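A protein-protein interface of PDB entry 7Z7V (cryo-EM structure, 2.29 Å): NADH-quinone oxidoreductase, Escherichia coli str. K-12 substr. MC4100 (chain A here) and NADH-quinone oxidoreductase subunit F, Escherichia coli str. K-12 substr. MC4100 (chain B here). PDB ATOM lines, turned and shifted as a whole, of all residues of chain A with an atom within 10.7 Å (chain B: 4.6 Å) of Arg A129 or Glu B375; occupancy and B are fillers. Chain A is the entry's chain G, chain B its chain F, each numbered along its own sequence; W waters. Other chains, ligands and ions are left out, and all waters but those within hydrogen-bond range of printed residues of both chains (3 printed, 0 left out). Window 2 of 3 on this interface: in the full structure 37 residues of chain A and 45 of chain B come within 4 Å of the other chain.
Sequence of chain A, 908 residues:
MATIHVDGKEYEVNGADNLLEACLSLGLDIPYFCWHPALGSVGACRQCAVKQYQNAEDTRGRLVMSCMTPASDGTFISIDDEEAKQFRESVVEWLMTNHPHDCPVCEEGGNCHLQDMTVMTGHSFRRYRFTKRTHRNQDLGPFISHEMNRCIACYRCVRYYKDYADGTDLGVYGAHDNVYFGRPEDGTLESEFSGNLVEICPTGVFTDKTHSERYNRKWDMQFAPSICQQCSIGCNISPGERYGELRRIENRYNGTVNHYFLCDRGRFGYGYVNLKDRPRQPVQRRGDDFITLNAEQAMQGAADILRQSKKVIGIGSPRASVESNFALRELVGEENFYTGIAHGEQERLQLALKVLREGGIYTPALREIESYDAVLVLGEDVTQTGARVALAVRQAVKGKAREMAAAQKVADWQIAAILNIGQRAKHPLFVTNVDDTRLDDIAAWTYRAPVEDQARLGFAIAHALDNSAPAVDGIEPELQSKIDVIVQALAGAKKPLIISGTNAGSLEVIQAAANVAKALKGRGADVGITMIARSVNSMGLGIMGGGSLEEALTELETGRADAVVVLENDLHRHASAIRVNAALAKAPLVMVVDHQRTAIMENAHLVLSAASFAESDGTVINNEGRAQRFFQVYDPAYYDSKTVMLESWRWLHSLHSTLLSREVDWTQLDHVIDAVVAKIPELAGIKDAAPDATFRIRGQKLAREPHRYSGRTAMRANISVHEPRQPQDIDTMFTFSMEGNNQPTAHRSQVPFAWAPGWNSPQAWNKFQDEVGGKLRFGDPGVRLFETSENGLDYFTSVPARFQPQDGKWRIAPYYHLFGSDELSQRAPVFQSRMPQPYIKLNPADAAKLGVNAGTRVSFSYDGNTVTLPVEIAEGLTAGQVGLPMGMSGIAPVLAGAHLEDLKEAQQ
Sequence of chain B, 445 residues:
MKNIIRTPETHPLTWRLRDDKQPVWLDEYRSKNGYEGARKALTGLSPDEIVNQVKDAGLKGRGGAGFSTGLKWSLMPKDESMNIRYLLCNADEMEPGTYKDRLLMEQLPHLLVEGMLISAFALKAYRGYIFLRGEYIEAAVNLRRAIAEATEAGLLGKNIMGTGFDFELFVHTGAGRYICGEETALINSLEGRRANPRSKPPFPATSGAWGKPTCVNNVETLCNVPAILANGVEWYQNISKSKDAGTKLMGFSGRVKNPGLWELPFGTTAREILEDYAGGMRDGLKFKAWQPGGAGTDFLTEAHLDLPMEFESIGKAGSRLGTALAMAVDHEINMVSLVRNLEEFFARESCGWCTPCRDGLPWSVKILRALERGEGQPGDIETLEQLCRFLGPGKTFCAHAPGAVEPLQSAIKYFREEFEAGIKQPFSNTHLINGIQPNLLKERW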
ATOM      1  N   GLU A  93       1.665   7.159  20.856  1.00  0.00           N
ATOM      2  CA  GLU A  93       3.035   7.523  20.501  1.00  0.00           C
ATOM      3  C   GLU A  93       3.459   8.838  21.147  1.00  0.00           C
ATOM      4  O   GLU A  93       4.591   8.962  21.626  1.00  0.00           O
ATOM      5  CB  GLU A  93       3.170   7.611  18.981  1.00  0.00           C
ATOM      6  CG  GLU A  93       4.522   8.101  18.508  1.00  0.00           C
ATOM      7  CD  GLU A  93       4.749   7.861  17.037  1.00  0.00           C
ATOM      8  OE1 GLU A  93       3.875   8.229  16.229  1.00  0.00           O
ATOM      9  OE2 GLU A  93       5.806   7.301  16.685  1.00  0.00           O
ATOM     10  N   MET A  96       4.250   8.229  24.564  1.00  0.00           N
ATOM     11  CA  MET A  96       5.476   7.453  24.663  1.00  0.00           C
ATOM     12  C   MET A  96       6.741   8.280  24.475  1.00  0.00           C
ATOM     13  O   MET A  96       7.824   7.775  24.781  1.00  0.00           O
ATOM     14  CB  MET A  96       5.462   6.325  23.629  1.00  0.00           C
ATOM     15  CG  MET A  96       4.673   5.110  24.056  1.00  0.00           C
ATOM     16  SD  MET A  96       5.226   4.488  25.647  1.00  0.00           S
ATOM     17  CE  MET A  96       3.690   4.544  26.550  1.00  0.00           C
ATOM     18  N   THR A  97       6.637   9.516  23.975  1.00  0.00           N
ATOM     19  CA  THR A  97       7.833  10.303  23.680  1.00  0.00           C
ATOM     20  C   THR A  97       8.610  10.635  24.947  1.00  0.00           C
ATOM     21  O   THR A  97       9.845  10.608  24.949  1.00  0.00           O
ATOM     22  CB  THR A  97       7.467  11.588  22.935  1.00  0.00           C
ATOM     23  OG1 THR A  97       6.459  12.303  23.656  1.00  0.00           O
ATOM     24  CG2 THR A  97       6.962  11.277  21.542  1.00  0.00           C
ATOM     25  N   ASN A  98       7.911  10.933  26.035  1.00  0.00           N
ATOM     26  CA  ASN A  98       8.551  11.304  27.286  1.00  0.00           C
ATOM     27  C   ASN A  98       8.524  10.203  28.335  1.00  0.00           C
ATOM     28  O   ASN A  98       9.011  10.423  29.445  1.00  0.00           O
ATOM     29  CB  ASN A  98       7.888  12.556  27.857  1.00  0.00           C
ATOM     30  CG  ASN A  98       8.069  13.759  26.972  1.00  0.00           C
ATOM     31  OD1 ASN A  98       9.190  14.152  26.661  1.00  0.00           O
ATOM     32  ND2 ASN A  98       6.963  14.357  26.560  1.00  0.00           N
ATOM     33  N   HIS A 123       1.075   0.115  18.835  1.00  0.00           N
ATOM     34  CA  HIS A 123       2.274   0.940  18.754  1.00  0.00           C
ATOM     35  C   HIS A 123       3.427   0.207  19.429  1.00  0.00           C
ATOM     36  O   HIS A 123       3.425   0.019  20.648  1.00  0.00           O
ATOM     37  CB  HIS A 123       2.039   2.298  19.404  1.00  0.00           C
ATOM     38  CG  HIS A 123       3.233   3.196  19.361  1.00  0.00           C
ATOM     39  ND1 HIS A 123       3.679   3.783  18.197  1.00  0.00           N
ATOM     40  CD2 HIS A 123       4.084   3.595  20.333  1.00  0.00           C
ATOM     41  CE1 HIS A 123       4.749   4.509  18.457  1.00  0.00           C
ATOM     42  NE2 HIS A 123       5.017   4.412  19.746  1.00  0.00           N
ATOM     43  N   PHE A 125       6.854   0.582  17.662  1.00  0.00           N
ATOM     44  CA  PHE A 125       8.039   1.093  16.987  1.00  0.00           C
ATOM     45  C   PHE A 125       8.220   2.555  17.362  1.00  0.00           C
ATOM     46  O   PHE A 125       7.313   3.366  17.154  1.00  0.00           O
ATOM     47  CB  PHE A 125       7.906   0.931  15.471  1.00  0.00           C
ATOM     48  CG  PHE A 125       9.150   1.269  14.710  1.00  0.00           C
ATOM     49  CD1 PHE A 125      10.149   0.327  14.538  1.00  0.00           C
ATOM     50  CD2 PHE A 125       9.320   2.529  14.158  1.00  0.00           C
ATOM     51  CE1 PHE A 125      11.298   0.636  13.833  1.00  0.00           C
ATOM     52  CE2 PHE A 125      10.466   2.843  13.455  1.00  0.00           C
ATOM     53  CZ  PHE A 125      11.456   1.894  13.293  1.00  0.00           C
ATOM     54  N   ARG A 126       9.391   2.894  17.886  1.00  0.00           N
ATOM     55  CA  ARG A 126       9.706   4.255  18.296  1.00  0.00           C
ATOM     56  C   ARG A 126      10.448   4.961  17.171  1.00  0.00           C
ATOM     57  O   ARG A 126      11.502   4.492  16.731  1.00  0.00           O
ATOM     58  CB  ARG A 126      10.553   4.255  19.568  1.00  0.00           C
ATOM     59  CG  ARG A 126      10.800   5.629  20.162  1.00  0.00           C
ATOM     60  CD  ARG A 126      11.567   5.515  21.460  1.00  0.00           C
ATOM     61  NE  ARG A 126      11.763   6.800  22.117  1.00  0.00           N
ATOM     62  CZ  ARG A 126      10.885   7.372  22.928  1.00  0.00           C
ATOM     63  NH1 ARG A 126       9.716   6.814  23.183  1.00  0.00           N
ATOM     64  NH2 ARG A 126      11.186   8.533  23.496  1.00  0.00           N
ATOM     65  N   ARG A 127       9.909   6.088  16.713  1.00  0.00           N
ATOM     66  CA  ARG A 127      10.620   6.941  15.773  1.00  0.00           C
ATOM     67  C   ARG A 127      11.014   8.285  16.365  1.00  0.00           C
ATOM     68  O   ARG A 127      11.789   9.013  15.738  1.00  0.00           O
ATOM     69  CB  ARG A 127       9.787   7.165  14.504  1.00  0.00           C
ATOM     70  CG  ARG A 127       8.457   7.827  14.731  1.00  0.00           C
ATOM     71  CD  ARG A 127       7.421   7.285  13.768  1.00  0.00           C
ATOM     72  NE  ARG A 127       6.103   7.840  14.038  1.00  0.00           N
ATOM     73  CZ  ARG A 127       5.535   8.799  13.322  1.00  0.00           C
ATOM     74  NH1 ARG A 127       6.131   9.312  12.259  1.00  0.00           N
ATOM     75  NH2 ARG A 127       4.338   9.252  13.680  1.00  0.00           N
ATOM     76  N   TYR A 128      10.504   8.630  17.542  1.00  0.00           N
ATOM     77  CA  TYR A 128      10.961   9.812  18.258  1.00  0.00           C
ATOM     78  C   TYR A 128      12.390   9.599  18.739  1.00  0.00           C
ATOM     79  O   TYR A 128      12.715   8.551  19.303  1.00  0.00           O
ATOM     80  CB  TYR A 128      10.027  10.084  19.435  1.00  0.00           C
ATOM     81  CG  TYR A 128      10.377  11.268  20.298  1.00  0.00           C
ATOM     82  CD1 TYR A 128       9.964  12.548  19.958  1.00  0.00           C
ATOM     83  CD2 TYR A 128      11.095  11.101  21.474  1.00  0.00           C
ATOM     84  CE1 TYR A 128      10.269  13.626  20.758  1.00  0.00           C
ATOM     85  CE2 TYR A 128      11.406  12.170  22.275  1.00  0.00           C
ATOM     86  CZ  TYR A 128      10.990  13.430  21.914  1.00  0.00           C
ATOM     87  OH  TYR A 128      11.303  14.495  22.718  1.00  0.00           O
ATOM     88  N   ARG A 129      13.249  10.594  18.522  1.00  0.00           N
ATOM     89  CA  ARG A 129      14.670  10.447  18.796  1.00  0.00           C
ATOM     90  C   ARG A 129      15.232  11.491  19.747  1.00  0.00           C
ATOM     91  O   ARG A 129      16.434  11.460  20.030  1.00  0.00           O
ATOM     92  CB  ARG A 129      15.464  10.481  17.484  1.00  0.00           C
ATOM     93  CG  ARG A 129      15.599  11.861  16.868  1.00  0.00           C
ATOM     94  CD  ARG A 129      16.504  11.819  15.656  1.00  0.00           C
ATOM     95  NE  ARG A 129      16.644  13.117  15.010  1.00  0.00           N
ATOM     96  CZ  ARG A 129      15.815  13.590  14.090  1.00  0.00           C
ATOM     97  NH1 ARG A 129      14.750  12.909  13.704  1.00  0.00           N
ATOM     98  NH2 ARG A 129      16.060  14.777  13.545  1.00  0.00           N
ATOM     99  N   PHE A 130      14.416  12.395  20.255  1.00  0.00           N
ATOM    100  CA  PHE A 130      14.897  13.514  21.039  1.00  0.00           C
ATOM    101  C   PHE A 130      14.821  13.185  22.529  1.00  0.00           C
ATOM    102  O   PHE A 130      14.590  12.041  22.924  1.00  0.00           O
ATOM    103  CB  PHE A 130      14.107  14.760  20.650  1.00  0.00           C
ATOM    104  CG  PHE A 130      14.093  15.020  19.170  1.00  0.00           C
ATOM    105  CD1 PHE A 130      15.198  15.568  18.541  1.00  0.00           C
ATOM    106  CD2 PHE A 130      12.984  14.701  18.405  1.00  0.00           C
ATOM    107  CE1 PHE A 130      15.194  15.801  17.181  1.00  0.00           C
ATOM    108  CE2 PHE A 130      12.974  14.933  17.043  1.00  0.00           C
ATOM    109  CZ  PHE A 130      14.081  15.486  16.432  1.00  0.00           C
ATOM    110  N   THR A 131      15.039  14.190  23.371  1.00  0.00           N
ATOM    111  CA  THR A 131      15.118  13.970  24.805  1.00  0.00           C
ATOM    112  C   THR A 131      13.732  13.775  25.415  1.00  0.00           C
ATOM    113  O   THR A 131      12.713  14.189  24.863  1.00  0.00           O
ATOM    114  CB  THR A 131      15.820  15.137  25.498  1.00  0.00           C
ATOM    115  OG1 THR A 131      15.102  16.350  25.243  1.00  0.00           O
ATOM    116  CG2 THR A 131      17.238  15.281  24.990  1.00  0.00           C
ATOM    117  N   LYS A 132      13.717  13.133  26.576  1.00  0.00           N
ATOM    118  CA  LYS A 132      12.506  12.942  27.358  1.00  0.00           C
ATOM    119  C   LYS A 132      12.514  13.892  28.545  1.00  0.00           C
ATOM    120  O   LYS A 132      13.544  14.071  29.200  1.00  0.00           O
ATOM    121  CB  LYS A 132      12.390  11.499  27.853  1.00  0.00           C
ATOM    122  CG  LYS A 132      12.648  10.450  26.794  1.00  0.00           C
ATOM    123  CD  LYS A 132      12.075   9.107  27.206  1.00  0.00           C
ATOM    124  CE  LYS A 132      13.166   8.121  27.560  1.00  0.00           C
ATOM    125  NZ  LYS A 132      12.638   6.744  27.740  1.00  0.00           N
ATOM    126  N   ARG A 133      11.367  14.510  28.811  1.00  0.00           N
ATOM    127  CA  ARG A 133      11.246  15.358  29.983  1.00  0.00           C
ATOM    128  C   ARG A 133      11.305  14.515  31.253  1.00  0.00           C
ATOM    129  O   ARG A 133      10.937  13.338  31.265  1.00  0.00           O
ATOM    130  CB  ARG A 133       9.950  16.172  29.942  1.00  0.00           C
ATOM    131  CG  ARG A 133       8.672  15.365  30.059  1.00  0.00           C
ATOM    132  CD  ARG A 133       8.042  15.504  31.434  1.00  0.00           C
ATOM    133  NE  ARG A 133       6.901  14.617  31.625  1.00  0.00           N
ATOM    134  CZ  ARG A 133       6.983  13.326  31.921  1.00  0.00           C
ATOM    135  NH1 ARG A 133       8.149  12.715  32.041  1.00  0.00           N
ATOM    136  NH2 ARG A 133       5.866  12.632  32.098  1.00  0.00           N
ATOM    137  N   ALA B 370      16.107  20.715  14.782  1.00  0.00           N
ATOM    138  CA  ALA B 370      17.075  19.875  14.081  1.00  0.00           C
ATOM    139  C   ALA B 370      17.220  20.288  12.620  1.00  0.00           C
ATOM    140  O   ALA B 370      18.331  20.299  12.083  1.00  0.00           O
ATOM    141  CB  ALA B 370      16.670  18.407  14.188  1.00  0.00           C
ATOM    142  N   ARG B 373      19.577  23.532  12.071  1.00  0.00           N
ATOM    143  CA  ARG B 373      21.024  23.366  12.056  1.00  0.00           C
ATOM    144  C   ARG B 373      21.473  22.230  11.147  1.00  0.00           C
ATOM    145  O   ARG B 373      22.608  21.758  11.269  1.00  0.00           O
ATOM    146  CB  ARG B 373      21.555  23.149  13.474  1.00  0.00           C
ATOM    147  CG  ARG B 373      20.593  22.466  14.406  1.00  0.00           C
ATOM    148  CD  ARG B 373      21.195  22.255  15.785  1.00  0.00           C
ATOM    149  NE  ARG B 373      20.177  22.224  16.828  1.00  0.00           N
ATOM    150  CZ  ARG B 373      19.437  21.163  17.130  1.00  0.00           C
ATOM    151  NH1 ARG B 373      19.580  20.015  16.490  1.00  0.00           N
ATOM    152  NH2 ARG B 373      18.532  21.258  18.100  1.00  0.00           N
ATOM    153  N   GLY B 374      20.609  21.778  10.243  1.00  0.00           N
ATOM    154  CA  GLY B 374      20.986  20.733   9.314  1.00  0.00           C
ATOM    155  C   GLY B 374      21.123  19.361   9.923  1.00  0.00           C
ATOM    156  O   GLY B 374      21.822  18.515   9.365  1.00  0.00           O
ATOM    157  N   GLU B 375      20.478  19.113  11.061  1.00  0.00           N
ATOM    158  CA  GLU B 375      20.538  17.823  11.730  1.00  0.00           C
ATOM    159  C   GLU B 375      19.289  16.988  11.486  1.00  0.00           C
ATOM    160  O   GLU B 375      19.055  16.012  12.204  1.00  0.00           O
ATOM    161  CB  GLU B 375      20.764  18.019  13.228  1.00  0.00           C
ATOM    162  CG  GLU B 375      22.215  18.246  13.597  1.00  0.00           C
ATOM    163  CD  GLU B 375      22.385  19.056  14.859  1.00  0.00           C
ATOM    164  OE1 GLU B 375      21.553  18.910  15.779  1.00  0.00           O
ATOM    165  OE2 GLU B 375      23.355  19.838  14.935  1.00  0.00           O
ATOM    166  N   GLY B 376      18.479  17.361  10.500  1.00  0.00           N
ATOM    167  CA  GLY B 376      17.290  16.598  10.193  1.00  0.00           C
ATOM    168  C   GLY B 376      17.609  15.243   9.592  1.00  0.00           C
ATOM    169  O   GLY B 376      18.665  15.015   9.005  1.00  0.00           O
ATOM    170  N   GLN B 377      16.666  14.332   9.749  1.00  0.00           N
ATOM    171  CA  GLN B 377      16.790  12.944   9.336  1.00  0.00           C
ATOM    172  C   GLN B 377      15.578  12.585   8.493  1.00  0.00           C
ATOM    173  O   GLN B 377      14.549  13.265   8.569  1.00  0.00           O
ATOM    174  CB  GLN B 377      16.904  12.028  10.565  1.00  0.00           C
ATOM    175  CG  GLN B 377      18.193  12.241  11.343  1.00  0.00           C
ATOM    176  CD  GLN B 377      18.308  11.354  12.561  1.00  0.00           C
ATOM    177  OE1 GLN B 377      17.476  10.483  12.788  1.00  0.00           O
ATOM    178  NE2 GLN B 377      19.345  11.577  13.357  1.00  0.00           N
ATOM    179  N   ASP B 380      11.358  13.178   8.845  1.00  0.00           N
ATOM    180  CA  ASP B 380      11.023  14.322   9.688  1.00  0.00           C
ATOM    181  C   ASP B 380       9.898  15.153   9.086  1.00  0.00           C
ATOM    182  O   ASP B 380       8.989  15.587   9.803  1.00  0.00           O
ATOM    183  CB  ASP B 380      12.260  15.186   9.916  1.00  0.00           C
ATOM    184  CG  ASP B 380      13.110  14.693  11.066  1.00  0.00           C
ATOM    185  OD1 ASP B 380      12.716  13.704  11.714  1.00  0.00           O
ATOM    186  OD2 ASP B 380      14.170  15.295  11.326  1.00  0.00           O
ATOM    187  N   GLY B 422      17.271  20.886   5.319  1.00  0.00           N
ATOM    188  CA  GLY B 422      17.766  20.573   6.644  1.00  0.00           C
ATOM    189  C   GLY B 422      17.970  19.103   6.926  1.00  0.00           C
ATOM    190  O   GLY B 422      18.478  18.759   7.996  1.00  0.00           O
ATOM    191  N   GLN B 425      21.618  14.161   7.939  1.00  0.00           N
ATOM    192  CA  GLN B 425      22.017  12.902   8.542  1.00  0.00           C
ATOM    193  C   GLN B 425      21.010  11.796   8.231  1.00  0.00           C
ATOM    194  O   GLN B 425      19.825  12.066   8.033  1.00  0.00           O
ATOM    195  CB  GLN B 425      22.156  13.059  10.050  1.00  0.00           C
ATOM    196  CG  GLN B 425      22.437  14.468  10.505  1.00  0.00           C
ATOM    197  CD  GLN B 425      22.448  14.587  12.008  1.00  0.00           C
ATOM    198  OE1 GLN B 425      21.641  13.967  12.698  1.00  0.00           O
ATOM    199  NE2 GLN B 425      23.390  15.359  12.530  1.00  0.00           N
ATOM    200  N   SER B 428      18.670   7.701  12.620  1.00  0.00           N
ATOM    201  CA  SER B 428      19.270   6.878  13.662  1.00  0.00           C
ATOM    202  C   SER B 428      18.521   7.151  14.955  1.00  0.00           C
ATOM    203  O   SER B 428      18.649   8.231  15.537  1.00  0.00           O
ATOM    204  CB  SER B 428      20.759   7.170  13.824  1.00  0.00           C
ATOM    205  OG  SER B 428      21.278   6.502  14.961  1.00  0.00           O
ATOM    206  N   ASN B 429      17.731   6.177  15.388  1.00  0.00           N
ATOM    207  CA  ASN B 429      17.041   6.236  16.662  1.00  0.00           C
ATOM    208  C   ASN B 429      17.675   5.336  17.711  1.00  0.00           C
ATOM    209  O   ASN B 429      17.346   5.461  18.893  1.00  0.00           O
ATOM    210  CB  ASN B 429      15.570   5.842  16.478  1.00  0.00           C
ATOM    211  CG  ASN B 429      14.685   6.423  17.536  1.00  0.00           C
ATOM    212  OD1 ASN B 429      15.123   7.247  18.328  1.00  0.00           O
ATOM    213  ND2 ASN B 429      13.437   5.993  17.567  1.00  0.00           N
HETATM  214  O   HOH W   1      18.801  15.386  14.870  1.00  0.00           O
HETATM  215  O   HOH W   2      14.430   7.802  21.370  1.00  0.00           O
HETATM  216  O   HOH W   3      17.930   8.744  19.861  1.00  0.00           O
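The side-chain carboxylate (OD1) of Asp B380 is in salt-bridge range of the guanidinium group (NH1) of Arg A129 (3.0 Å). The backbone carbonyl oxygen of Arg A126 lies within hydrogen-bond range of the side-chain amide nitrogen of Asn B429 (2.6 Å). OD1 of Asn B429 lies close to O of Tyr A128, 2.9 Å away.
The backbone carbonyl oxygen of Ala B370 sits at hydrogen-bond distance from the backbone NH of Glu B375 (2.7 Å). The backbone carbonyl oxygen (O) of Ala B370 sits at hydrogen-bond distance from the backbone NH (N) of Gly B376 (3.3 Å). O of Glu B375 lies close to OE1 of Gln B425, at 3.3 Å. The backbone NH (N) of Gln B377 is in hydrogen-bond range of the side-chain carboxylate (OD2) of Asp B380 (3.1 Å). O of Met A96 lies within hydrogen-bond range of NH1 of Arg A126 (2.7 Å). O of Thr A97 is in hydrogen-bond range of NH2 of Arg A126, 2.9 Å away.
CA of Arg A127 touches ND2 of Asn B429 (3.5 Å). NH2 of Arg A129 touches CB of Ala B370, 3.7 Å away. Glu B375 touches Arg A129 (O to NH2, 3.5 Å). OE1 of Gln B377 touches CD of Arg A129, at 3.3 Å. Arg A129 touches Asn B429 (CA to OD1, 3.3 Å).
Of the printed residues of chain B, Arg A129 touches Ala B370, Glu B375, Gln B377, Asp B380 and Asn B429. No residue of chain A comes within 4 Å of Gly B374. Gln B377 touches just one residue of chain A: Arg A129 (3.3 Å). Of the printed residues of chain A, Asp B380 touches Arg A129 (3.0 Å). Of the printed residues of chain B, Tyr A128 touches Asn B429. The nearest printed residue of chain B that does not touch Arg A129 is Gly B376 (4.01 Å). The nearest residue of chain A that does not touch Glu B375 is Phe A130 (6.3 Å). The nearest printed residue of chain B that does not touch Tyr A128 is Ser B428 (7.0 Å).
Of the 14 printed residues of chain A, 4 touch a printed residue of chain B. Hydrophobic or aromatic side chains of chain B within 4 Å of the printed part of chain A: Ala B370. Among the printed residues, Asp or Glu carboxylates within 4 Å of a Lys or Arg side-chain nitrogen of the other chain: Arg A129 with Asp B380 (3.0 Å).
Water W1 bridges the backbone carbonyl oxygen of Glu B375 (2.8 Å) and the guanidinium group of Arg A129 (3.1 Å). Water W2 lies within hydrogen-bond range of O of Tyr A128, NE of Arg A126 and OD1 of Asn B429. Water W3 bridges the backbone carbonyl oxygen of Arg A129 and the backbone carbonyl oxygen of Asn B429.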
